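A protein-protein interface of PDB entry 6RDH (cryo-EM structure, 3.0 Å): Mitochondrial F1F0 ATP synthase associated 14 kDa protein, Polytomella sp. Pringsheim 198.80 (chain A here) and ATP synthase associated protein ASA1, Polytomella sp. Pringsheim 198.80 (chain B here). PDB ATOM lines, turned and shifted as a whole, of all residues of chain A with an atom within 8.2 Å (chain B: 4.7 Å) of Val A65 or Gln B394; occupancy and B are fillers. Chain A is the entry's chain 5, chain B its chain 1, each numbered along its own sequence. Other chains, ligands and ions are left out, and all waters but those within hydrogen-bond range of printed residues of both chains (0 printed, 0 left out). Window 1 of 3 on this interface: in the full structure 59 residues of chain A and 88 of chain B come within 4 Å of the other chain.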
ATOM      1  N   PRO A  60       5.432 -22.673   2.295  1.00  0.00           N
ATOM      2  CA  PRO A  60       5.456 -21.497   1.421  1.00  0.00           C
ATOM      3  C   PRO A  60       4.364 -21.455   0.369  1.00  0.00           C
ATOM      4  O   PRO A  60       4.484 -20.674  -0.576  1.00  0.00           O
ATOM      5  CB  PRO A  60       6.823 -21.637   0.754  1.00  0.00           C
ATOM      6  CG  PRO A  60       6.994 -23.090   0.630  1.00  0.00           C
ATOM      7  CD  PRO A  60       6.339 -23.722   1.804  1.00  0.00           C
ATOM      8  N   SER A  61       3.314 -22.253   0.508  1.00  0.00           N
ATOM      9  CA  SER A  61       2.359 -22.461  -0.562  1.00  0.00           C
ATOM     10  C   SER A  61       1.144 -21.568  -0.460  1.00  0.00           C
ATOM     11  O   SER A  61       0.056 -21.986  -0.861  1.00  0.00           O
ATOM     12  CB  SER A  61       1.928 -23.920  -0.594  1.00  0.00           C
ATOM     13  OG  SER A  61       1.345 -24.295   0.628  1.00  0.00           O
ATOM     14  N   TYR A  62       1.290 -20.362   0.068  1.00  0.00           N
ATOM     15  CA  TYR A  62       0.231 -19.364   0.013  1.00  0.00           C
ATOM     16  C   TYR A  62       0.601 -18.151  -0.811  1.00  0.00           C
ATOM     17  O   TYR A  62      -0.254 -17.582  -1.483  1.00  0.00           O
ATOM     18  CB  TYR A  62      -0.136 -18.898   1.412  1.00  0.00           C
ATOM     19  CG  TYR A  62      -0.418 -20.007   2.360  1.00  0.00           C
ATOM     20  CD1 TYR A  62      -1.494 -20.848   2.162  1.00  0.00           C
ATOM     21  CD2 TYR A  62       0.389 -20.217   3.453  1.00  0.00           C
ATOM     22  CE1 TYR A  62      -1.753 -21.865   3.026  1.00  0.00           C
ATOM     23  CE2 TYR A  62       0.134 -21.225   4.316  1.00  0.00           C
ATOM     24  CZ  TYR A  62      -0.936 -22.045   4.097  1.00  0.00           C
ATOM     25  OH  TYR A  62      -1.190 -23.059   4.962  1.00  0.00           O
ATOM     26  N   ASP A  63       1.863 -17.743  -0.752  1.00  0.00           N
ATOM     27  CA  ASP A  63       2.383 -16.615  -1.508  1.00  0.00           C
ATOM     28  C   ASP A  63       3.178 -17.081  -2.709  1.00  0.00           C
ATOM     29  O   ASP A  63       4.222 -16.517  -3.030  1.00  0.00           O
ATOM     30  CB  ASP A  63       3.239 -15.738  -0.609  1.00  0.00           C
ATOM     31  CG  ASP A  63       4.141 -16.548   0.295  1.00  0.00           C
ATOM     32  OD1 ASP A  63       4.091 -17.789   0.224  1.00  0.00           O
ATOM     33  OD2 ASP A  63       4.898 -15.946   1.083  1.00  0.00           O
ATOM     34  N   ARG A  64       2.721 -18.144  -3.369  1.00  0.00           N
ATOM     35  CA  ARG A  64       3.368 -18.603  -4.588  1.00  0.00           C
ATOM     36  C   ARG A  64       3.175 -17.631  -5.736  1.00  0.00           C
ATOM     37  O   ARG A  64       3.960 -17.657  -6.687  1.00  0.00           O
ATOM     38  CB  ARG A  64       2.822 -19.964  -5.002  1.00  0.00           C
ATOM     39  CG  ARG A  64       3.279 -21.108  -4.155  1.00  0.00           C
ATOM     40  CD  ARG A  64       4.774 -21.248  -4.194  1.00  0.00           C
ATOM     41  NE  ARG A  64       5.188 -22.582  -3.793  1.00  0.00           N
ATOM     42  CZ  ARG A  64       6.400 -22.877  -3.349  1.00  0.00           C
ATOM     43  NH1 ARG A  64       7.314 -21.928  -3.240  1.00  0.00           N
ATOM     44  NH2 ARG A  64       6.694 -24.116  -3.006  1.00  0.00           N
ATOM     45  N   VAL A  65       2.146 -16.785  -5.669  1.00  0.00           N
ATOM     46  CA  VAL A  65       1.908 -15.797  -6.706  1.00  0.00           C
ATOM     47  C   VAL A  65       2.963 -14.703  -6.684  1.00  0.00           C
ATOM     48  O   VAL A  65       3.221 -14.079  -7.715  1.00  0.00           O
ATOM     49  CB  VAL A  65       0.474 -15.250  -6.560  1.00  0.00           C
ATOM     50  CG1 VAL A  65       0.339 -14.329  -5.368  1.00  0.00           C
ATOM     51  CG2 VAL A  65       0.013 -14.573  -7.835  1.00  0.00           C
ATOM     52  N   LEU A  66       3.628 -14.483  -5.556  1.00  0.00           N
ATOM     53  CA  LEU A  66       4.655 -13.459  -5.513  1.00  0.00           C
ATOM     54  C   LEU A  66       5.981 -13.947  -6.064  1.00  0.00           C
ATOM     55  O   LEU A  66       6.901 -13.142  -6.224  1.00  0.00           O
ATOM     56  CB  LEU A  66       4.855 -12.962  -4.088  1.00  0.00           C
ATOM     57  CG  LEU A  66       3.625 -12.579  -3.281  1.00  0.00           C
ATOM     58  CD1 LEU A  66       4.070 -11.980  -1.981  1.00  0.00           C
ATOM     59  CD2 LEU A  66       2.763 -11.606  -4.024  1.00  0.00           C
ATOM     60  N   SER A  67       6.109 -15.236  -6.346  1.00  0.00           N
ATOM     61  CA  SER A  67       7.292 -15.737  -7.023  1.00  0.00           C
ATOM     62  C   SER A  67       7.169 -15.654  -8.531  1.00  0.00           C
ATOM     63  O   SER A  67       8.192 -15.674  -9.222  1.00  0.00           O
ATOM     64  CB  SER A  67       7.565 -17.186  -6.624  1.00  0.00           C
ATOM     65  OG  SER A  67       6.853 -18.080  -7.456  1.00  0.00           O
ATOM     66  N   LEU A  68       5.946 -15.574  -9.049  1.00  0.00           N
ATOM     67  CA  LEU A  68       5.713 -15.382 -10.465  1.00  0.00           C
ATOM     68  C   LEU A  68       6.141 -13.977 -10.873  1.00  0.00           C
ATOM     69  O   LEU A  68       6.216 -13.080 -10.030  1.00  0.00           O
ATOM     70  CB  LEU A  68       4.238 -15.590 -10.782  1.00  0.00           C
ATOM     71  CG  LEU A  68       3.676 -16.970 -10.500  1.00  0.00           C
ATOM     72  CD1 LEU A  68       2.226 -17.013 -10.902  1.00  0.00           C
ATOM     73  CD2 LEU A  68       4.464 -18.007 -11.245  1.00  0.00           C
ATOM     74  N   PRO A  69       6.457 -13.763 -12.153  1.00  0.00           N
ATOM     75  CA  PRO A  69       6.775 -12.403 -12.610  1.00  0.00           C
ATOM     76  C   PRO A  69       5.552 -11.504 -12.537  1.00  0.00           C
ATOM     77  O   PRO A  69       4.475 -11.856 -13.021  1.00  0.00           O
ATOM     78  CB  PRO A  69       7.237 -12.617 -14.052  1.00  0.00           C
ATOM     79  CG  PRO A  69       6.715 -13.948 -14.427  1.00  0.00           C
ATOM     80  CD  PRO A  69       6.769 -14.752 -13.195  1.00  0.00           C
ATOM     81  N   ALA A  70       5.728 -10.339 -11.905  1.00  0.00           N
ATOM     82  CA  ALA A  70       4.591  -9.490 -11.567  1.00  0.00           C
ATOM     83  C   ALA A  70       4.024  -8.789 -12.785  1.00  0.00           C
ATOM     84  O   ALA A  70       2.834  -8.456 -12.809  1.00  0.00           O
ATOM     85  CB  ALA A  70       4.993  -8.460 -10.519  1.00  0.00           C
ATOM     86  N   VAL A  71       4.851  -8.559 -13.797  1.00  0.00           N
ATOM     87  CA  VAL A  71       4.390  -7.934 -15.027  1.00  0.00           C
ATOM     88  C   VAL A  71       3.582  -8.950 -15.818  1.00  0.00           C
ATOM     89  O   VAL A  71       4.081 -10.026 -16.160  1.00  0.00           O
ATOM     90  CB  VAL A  71       5.573  -7.407 -15.837  1.00  0.00           C
ATOM     91  CG1 VAL A  71       5.113  -6.985 -17.197  1.00  0.00           C
ATOM     92  CG2 VAL A  71       6.207  -6.255 -15.114  1.00  0.00           C
ATOM     93  N   SER A  72       2.335  -8.605 -16.118  1.00  0.00           N
ATOM     94  CA  SER A  72       1.396  -9.514 -16.746  1.00  0.00           C
ATOM     95  C   SER A  72       1.804  -9.836 -18.177  1.00  0.00           C
ATOM     96  O   SER A  72       2.667  -9.193 -18.768  1.00  0.00           O
ATOM     97  CB  SER A  72       0.000  -8.909 -16.744  1.00  0.00           C
ATOM     98  OG  SER A  72      -0.926  -9.809 -17.310  1.00  0.00           O
ATOM     99  N   ASN A  74      -0.401  -9.461 -20.471  1.00  0.00           N
ATOM    100  CA  ASN A  74      -1.047  -8.339 -21.140  1.00  0.00           C
ATOM    101  C   ASN A  74      -0.132  -7.125 -21.196  1.00  0.00           C
ATOM    102  O   ASN A  74      -0.087  -6.421 -22.209  1.00  0.00           O
ATOM    103  CB  ASN A  74      -2.340  -8.006 -20.412  1.00  0.00           C
ATOM    104  CG  ASN A  74      -2.843  -6.641 -20.727  1.00  0.00           C
ATOM    105  OD1 ASN A  74      -3.104  -6.320 -21.876  1.00  0.00           O
ATOM    106  ND2 ASN A  74      -2.991  -5.817 -19.705  1.00  0.00           N
ATOM    107  N   PHE B 111      -1.647  -9.096  -1.903  1.00  0.00           N
ATOM    108  CA  PHE B 111      -0.949  -9.702  -3.032  1.00  0.00           C
ATOM    109  C   PHE B 111      -1.036  -8.824  -4.270  1.00  0.00           C
ATOM    110  O   PHE B 111      -0.061  -8.694  -5.016  1.00  0.00           O
ATOM    111  CB  PHE B 111      -1.530 -11.082  -3.326  1.00  0.00           C
ATOM    112  CG  PHE B 111      -1.147 -12.132  -2.332  1.00  0.00           C
ATOM    113  CD1 PHE B 111       0.010 -12.016  -1.589  1.00  0.00           C
ATOM    114  CD2 PHE B 111      -1.945 -13.239  -2.147  1.00  0.00           C
ATOM    115  CE1 PHE B 111       0.357 -12.985  -0.683  1.00  0.00           C
ATOM    116  CE2 PHE B 111      -1.602 -14.204  -1.240  1.00  0.00           C
ATOM    117  CZ  PHE B 111      -0.452 -14.076  -0.511  1.00  0.00           C
ATOM    118  N   ASP B 112      -2.185  -8.181  -4.474  1.00  0.00           N
ATOM    119  CA  ASP B 112      -2.359  -7.309  -5.625  1.00  0.00           C
ATOM    120  C   ASP B 112      -1.517  -6.051  -5.508  1.00  0.00           C
ATOM    121  O   ASP B 112      -0.957  -5.597  -6.505  1.00  0.00           O
ATOM    122  CB  ASP B 112      -3.826  -6.949  -5.795  1.00  0.00           C
ATOM    123  CG  ASP B 112      -4.658  -8.124  -6.218  1.00  0.00           C
ATOM    124  OD1 ASP B 112      -4.105  -9.045  -6.845  1.00  0.00           O
ATOM    125  OD2 ASP B 112      -5.863  -8.142  -5.907  1.00  0.00           O
ATOM    126  N   ILE B 115       2.153  -7.140  -6.192  1.00  0.00           N
ATOM    127  CA  ILE B 115       2.360  -7.431  -7.605  1.00  0.00           C
ATOM    128  C   ILE B 115       2.305  -6.157  -8.435  1.00  0.00           C
ATOM    129  O   ILE B 115       3.151  -5.938  -9.306  1.00  0.00           O
ATOM    130  CB  ILE B 115       1.324  -8.464  -8.071  1.00  0.00           C
ATOM    131  CG1 ILE B 115       1.684  -9.846  -7.546  1.00  0.00           C
ATOM    132  CG2 ILE B 115       1.236  -8.516  -9.568  1.00  0.00           C
ATOM    133  CD1 ILE B 115       0.551 -10.811  -7.647  1.00  0.00           C
ATOM    134  N   THR B 384      -9.440 -17.565 -16.682  1.00  0.00           N
ATOM    135  CA  THR B 384      -9.307 -16.457 -15.747  1.00  0.00           C
ATOM    136  C   THR B 384     -10.528 -16.333 -14.847  1.00  0.00           C
ATOM    137  O   THR B 384     -10.405 -15.954 -13.681  1.00  0.00           O
ATOM    138  CB  THR B 384      -9.072 -15.173 -16.527  1.00  0.00           C
ATOM    139  OG1 THR B 384      -8.059 -15.410 -17.507  1.00  0.00           O
ATOM    140  CG2 THR B 384      -8.610 -14.092 -15.632  1.00  0.00           C
ATOM    141  N   TYR B 388      -9.527 -16.899 -10.823  1.00  0.00           N
ATOM    142  CA  TYR B 388      -9.569 -15.652 -10.083  1.00  0.00           C
ATOM    143  C   TYR B 388     -11.002 -15.177  -9.938  1.00  0.00           C
ATOM    144  O   TYR B 388     -11.855 -15.452 -10.783  1.00  0.00           O
ATOM    145  CB  TYR B 388      -8.741 -14.570 -10.767  1.00  0.00           C
ATOM    146  CG  TYR B 388      -7.344 -15.006 -11.095  1.00  0.00           C
ATOM    147  CD1 TYR B 388      -6.374 -15.052 -10.114  1.00  0.00           C
ATOM    148  CD2 TYR B 388      -6.997 -15.382 -12.374  1.00  0.00           C
ATOM    149  CE1 TYR B 388      -5.096 -15.457 -10.400  1.00  0.00           C
ATOM    150  CE2 TYR B 388      -5.722 -15.790 -12.673  1.00  0.00           C
ATOM    151  CZ  TYR B 388      -4.776 -15.825 -11.681  1.00  0.00           C
ATOM    152  OH  TYR B 388      -3.500 -16.232 -11.971  1.00  0.00           O
ATOM    153  N   ARG B 392      -9.938  -9.263  -8.406  1.00  0.00           N
ATOM    154  CA  ARG B 392      -8.497  -9.441  -8.385  1.00  0.00           C
ATOM    155  C   ARG B 392      -7.820  -8.525  -9.388  1.00  0.00           C
ATOM    156  O   ARG B 392      -8.458  -7.874 -10.205  1.00  0.00           O
ATOM    157  CB  ARG B 392      -8.116 -10.885  -8.687  1.00  0.00           C
ATOM    158  CG  ARG B 392      -8.426 -11.856  -7.592  1.00  0.00           C
ATOM    159  CD  ARG B 392      -7.872 -11.434  -6.253  1.00  0.00           C
ATOM    160  NE  ARG B 392      -6.438 -11.653  -6.161  1.00  0.00           N
ATOM    161  CZ  ARG B 392      -5.881 -12.795  -5.786  1.00  0.00           C
ATOM    162  NH1 ARG B 392      -6.637 -13.831  -5.468  1.00  0.00           N
ATOM    163  NH2 ARG B 392      -4.564 -12.900  -5.731  1.00  0.00           N
ATOM    164  N   LEU B 393      -6.500  -8.481  -9.307  1.00  0.00           N
ATOM    165  CA  LEU B 393      -5.714  -7.802 -10.323  1.00  0.00           C
ATOM    166  C   LEU B 393      -5.458  -8.713 -11.508  1.00  0.00           C
ATOM    167  O   LEU B 393      -5.474  -8.269 -12.662  1.00  0.00           O
ATOM    168  CB  LEU B 393      -4.399  -7.328  -9.714  1.00  0.00           C
ATOM    169  CG  LEU B 393      -3.341  -6.696 -10.596  1.00  0.00           C
ATOM    170  CD1 LEU B 393      -2.829  -5.486  -9.901  1.00  0.00           C
ATOM    171  CD2 LEU B 393      -2.209  -7.656 -10.802  1.00  0.00           C
ATOM    172  N   GLN B 394      -5.222  -9.992 -11.236  1.00  0.00           N
ATOM    173  CA  GLN B 394      -4.919 -10.931 -12.298  1.00  0.00           C
ATOM    174  C   GLN B 394      -6.152 -11.291 -13.101  1.00  0.00           C
ATOM    175  O   GLN B 394      -6.017 -11.692 -14.253  1.00  0.00           O
ATOM    176  CB  GLN B 394      -4.273 -12.170 -11.705  1.00  0.00           C
ATOM    177  CG  GLN B 394      -3.304 -11.832 -10.601  1.00  0.00           C
ATOM    178  CD  GLN B 394      -2.137 -12.775 -10.547  1.00  0.00           C
ATOM    179  OE1 GLN B 394      -2.286 -13.943 -10.197  1.00  0.00           O
ATOM    180  NE2 GLN B 394      -0.963 -12.281 -10.907  1.00  0.00           N
ATOM    181  N   TYR B 395      -7.344 -11.098 -12.539  1.00  0.00           N
ATOM    182  CA  TYR B 395      -8.567 -11.226 -13.319  1.00  0.00           C
ATOM    183  C   TYR B 395      -8.651 -10.134 -14.369  1.00  0.00           C
ATOM    184  O   TYR B 395      -8.974 -10.399 -15.534  1.00  0.00           O
ATOM    185  CB  TYR B 395      -9.775 -11.164 -12.398  1.00  0.00           C
ATOM    186  CG  TYR B 395     -11.106 -11.388 -13.060  1.00  0.00           C
ATOM    187  CD1 TYR B 395     -11.593 -12.661 -13.251  1.00  0.00           C
ATOM    188  CD2 TYR B 395     -11.895 -10.323 -13.458  1.00  0.00           C
ATOM    189  CE1 TYR B 395     -12.813 -12.872 -13.837  1.00  0.00           C
ATOM    190  CE2 TYR B 395     -13.121 -10.528 -14.045  1.00  0.00           C
ATOM    191  CZ  TYR B 395     -13.571 -11.807 -14.228  1.00  0.00           C
ATOM    192  OH  TYR B 395     -14.789 -12.025 -14.813  1.00  0.00           O
ATOM    193  N   LYS B 396      -8.361  -8.897 -13.968  1.00  0.00           N
ATOM    194  CA  LYS B 396      -8.364  -7.780 -14.901  1.00  0.00           C
ATOM    195  C   LYS B 396      -7.302  -7.949 -15.974  1.00  0.00           C
ATOM    196  O   LYS B 396      -7.575  -7.739 -17.161  1.00  0.00           O
ATOM    197  CB  LYS B 396      -8.160  -6.480 -14.138  1.00  0.00           C
ATOM    198  CG  LYS B 396      -9.209  -6.263 -13.083  1.00  0.00           C
ATOM    199  CD  LYS B 396      -8.810  -5.191 -12.107  1.00  0.00           C
ATOM    200  CE  LYS B 396      -9.900  -5.002 -11.081  1.00  0.00           C
ATOM    201  NZ  LYS B 396      -9.481  -4.079 -10.002  1.00  0.00           N
ATOM    202  N   GLU B 397      -6.100  -8.369 -15.583  1.00  0.00           N
ATOM    203  CA  GLU B 397      -5.051  -8.568 -16.574  1.00  0.00           C
ATOM    204  C   GLU B 397      -5.341  -9.754 -17.488  1.00  0.00           C
ATOM    205  O   GLU B 397      -4.991  -9.716 -18.670  1.00  0.00           O
ATOM    206  CB  GLU B 397      -3.708  -8.739 -15.882  1.00  0.00           C
ATOM    207  CG  GLU B 397      -3.304  -7.554 -15.045  1.00  0.00           C
ATOM    208  CD  GLU B 397      -2.900  -6.356 -15.869  1.00  0.00           C
ATOM    209  OE1 GLU B 397      -2.281  -6.543 -16.930  1.00  0.00           O
ATOM    210  OE2 GLU B 397      -3.197  -5.219 -15.452  1.00  0.00           O
ATOM    211  N   GLY B 398      -6.016 -10.787 -16.987  1.00  0.00           N
ATOM    212  CA  GLY B 398      -6.369 -11.902 -17.844  1.00  0.00           C
ATOM    213  C   GLY B 398      -7.452 -11.548 -18.840  1.00  0.00           C
ATOM    214  O   GLY B 398      -7.423 -11.999 -19.986  1.00  0.00           O
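Of the 14 printed residues of chain A, 7 touch a printed residue of chain B.
Printed residues of chain A that touch a printed residue of chain B: Tyr A62, Asp A63, Val A65, Leu A66, Ala A70, Ser A72 and Asn A74.
Hydrophobic or aromatic side chains of chain A that line the printed part of chain B: Val A65, Leu A66 and Ala A70.
Of the 12 printed residues of chain B, 4 touch a printed residue of chain A.
Along chain B the printed residues that touch a printed residue of chain A span positions 111 to 397.
Among the printed residues, no Asp or Glu carboxylate lies within 4 Å of a Lys or Arg side-chain nitrogen of the other chain.
Tyr A62 touches Phe B111 (O to CZ, 3.6 Å).
Asp A63 touches Phe B111.
Val A65 touches Ile B115.
CG2 of Val A65 touches OE1 of Gln B394 (3.4 Å).
CD1 of Phe B111 touches CD2 of Leu A66 (3.7 Å).
Ile B115 touches Ala A70 (O to CB, 3.4 Å).
Glu B397 touches Ser A72 (OE1 to CB, 3.3 Å).
The side-chain carboxylate (OE1) of Glu B397 sits at hydrogen-bond distance from the side-chain amide nitrogen (ND2) of Asn A74.
Arg A64 touches none of the printed residues of chain B.
Val A65 touches just these residues of chain B: Ile B115 and Gln B394.
Printed residues of chain B within 4 Å of Leu A66: Phe B111 (3.7 Å).
Of the printed residues of chain B, Ala A70 touches Ile B115 (3.4 Å).
Of the printed residues of chain B, Asn A74 touches Glu B397.
Of the printed residues of chain A, Ile B115 touches Val A65 and Ala A70.
Tyr B388 touches none of the printed residues of chain A.
Gln B394 touches just one residue of chain A: Val A65.
The nearest printed residue of chain B that does not touch Asn A74 is Lys B396 (5.6 Å).
The side-chain hydroxyl (OH) of Tyr B388 sits at hydrogen-bond distance from the side-chain amide oxygen (OE1) of Gln B394, 3.1 Å away.
OG of Ser A72 sits close to N of Asn A74, at 3.2 Å.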
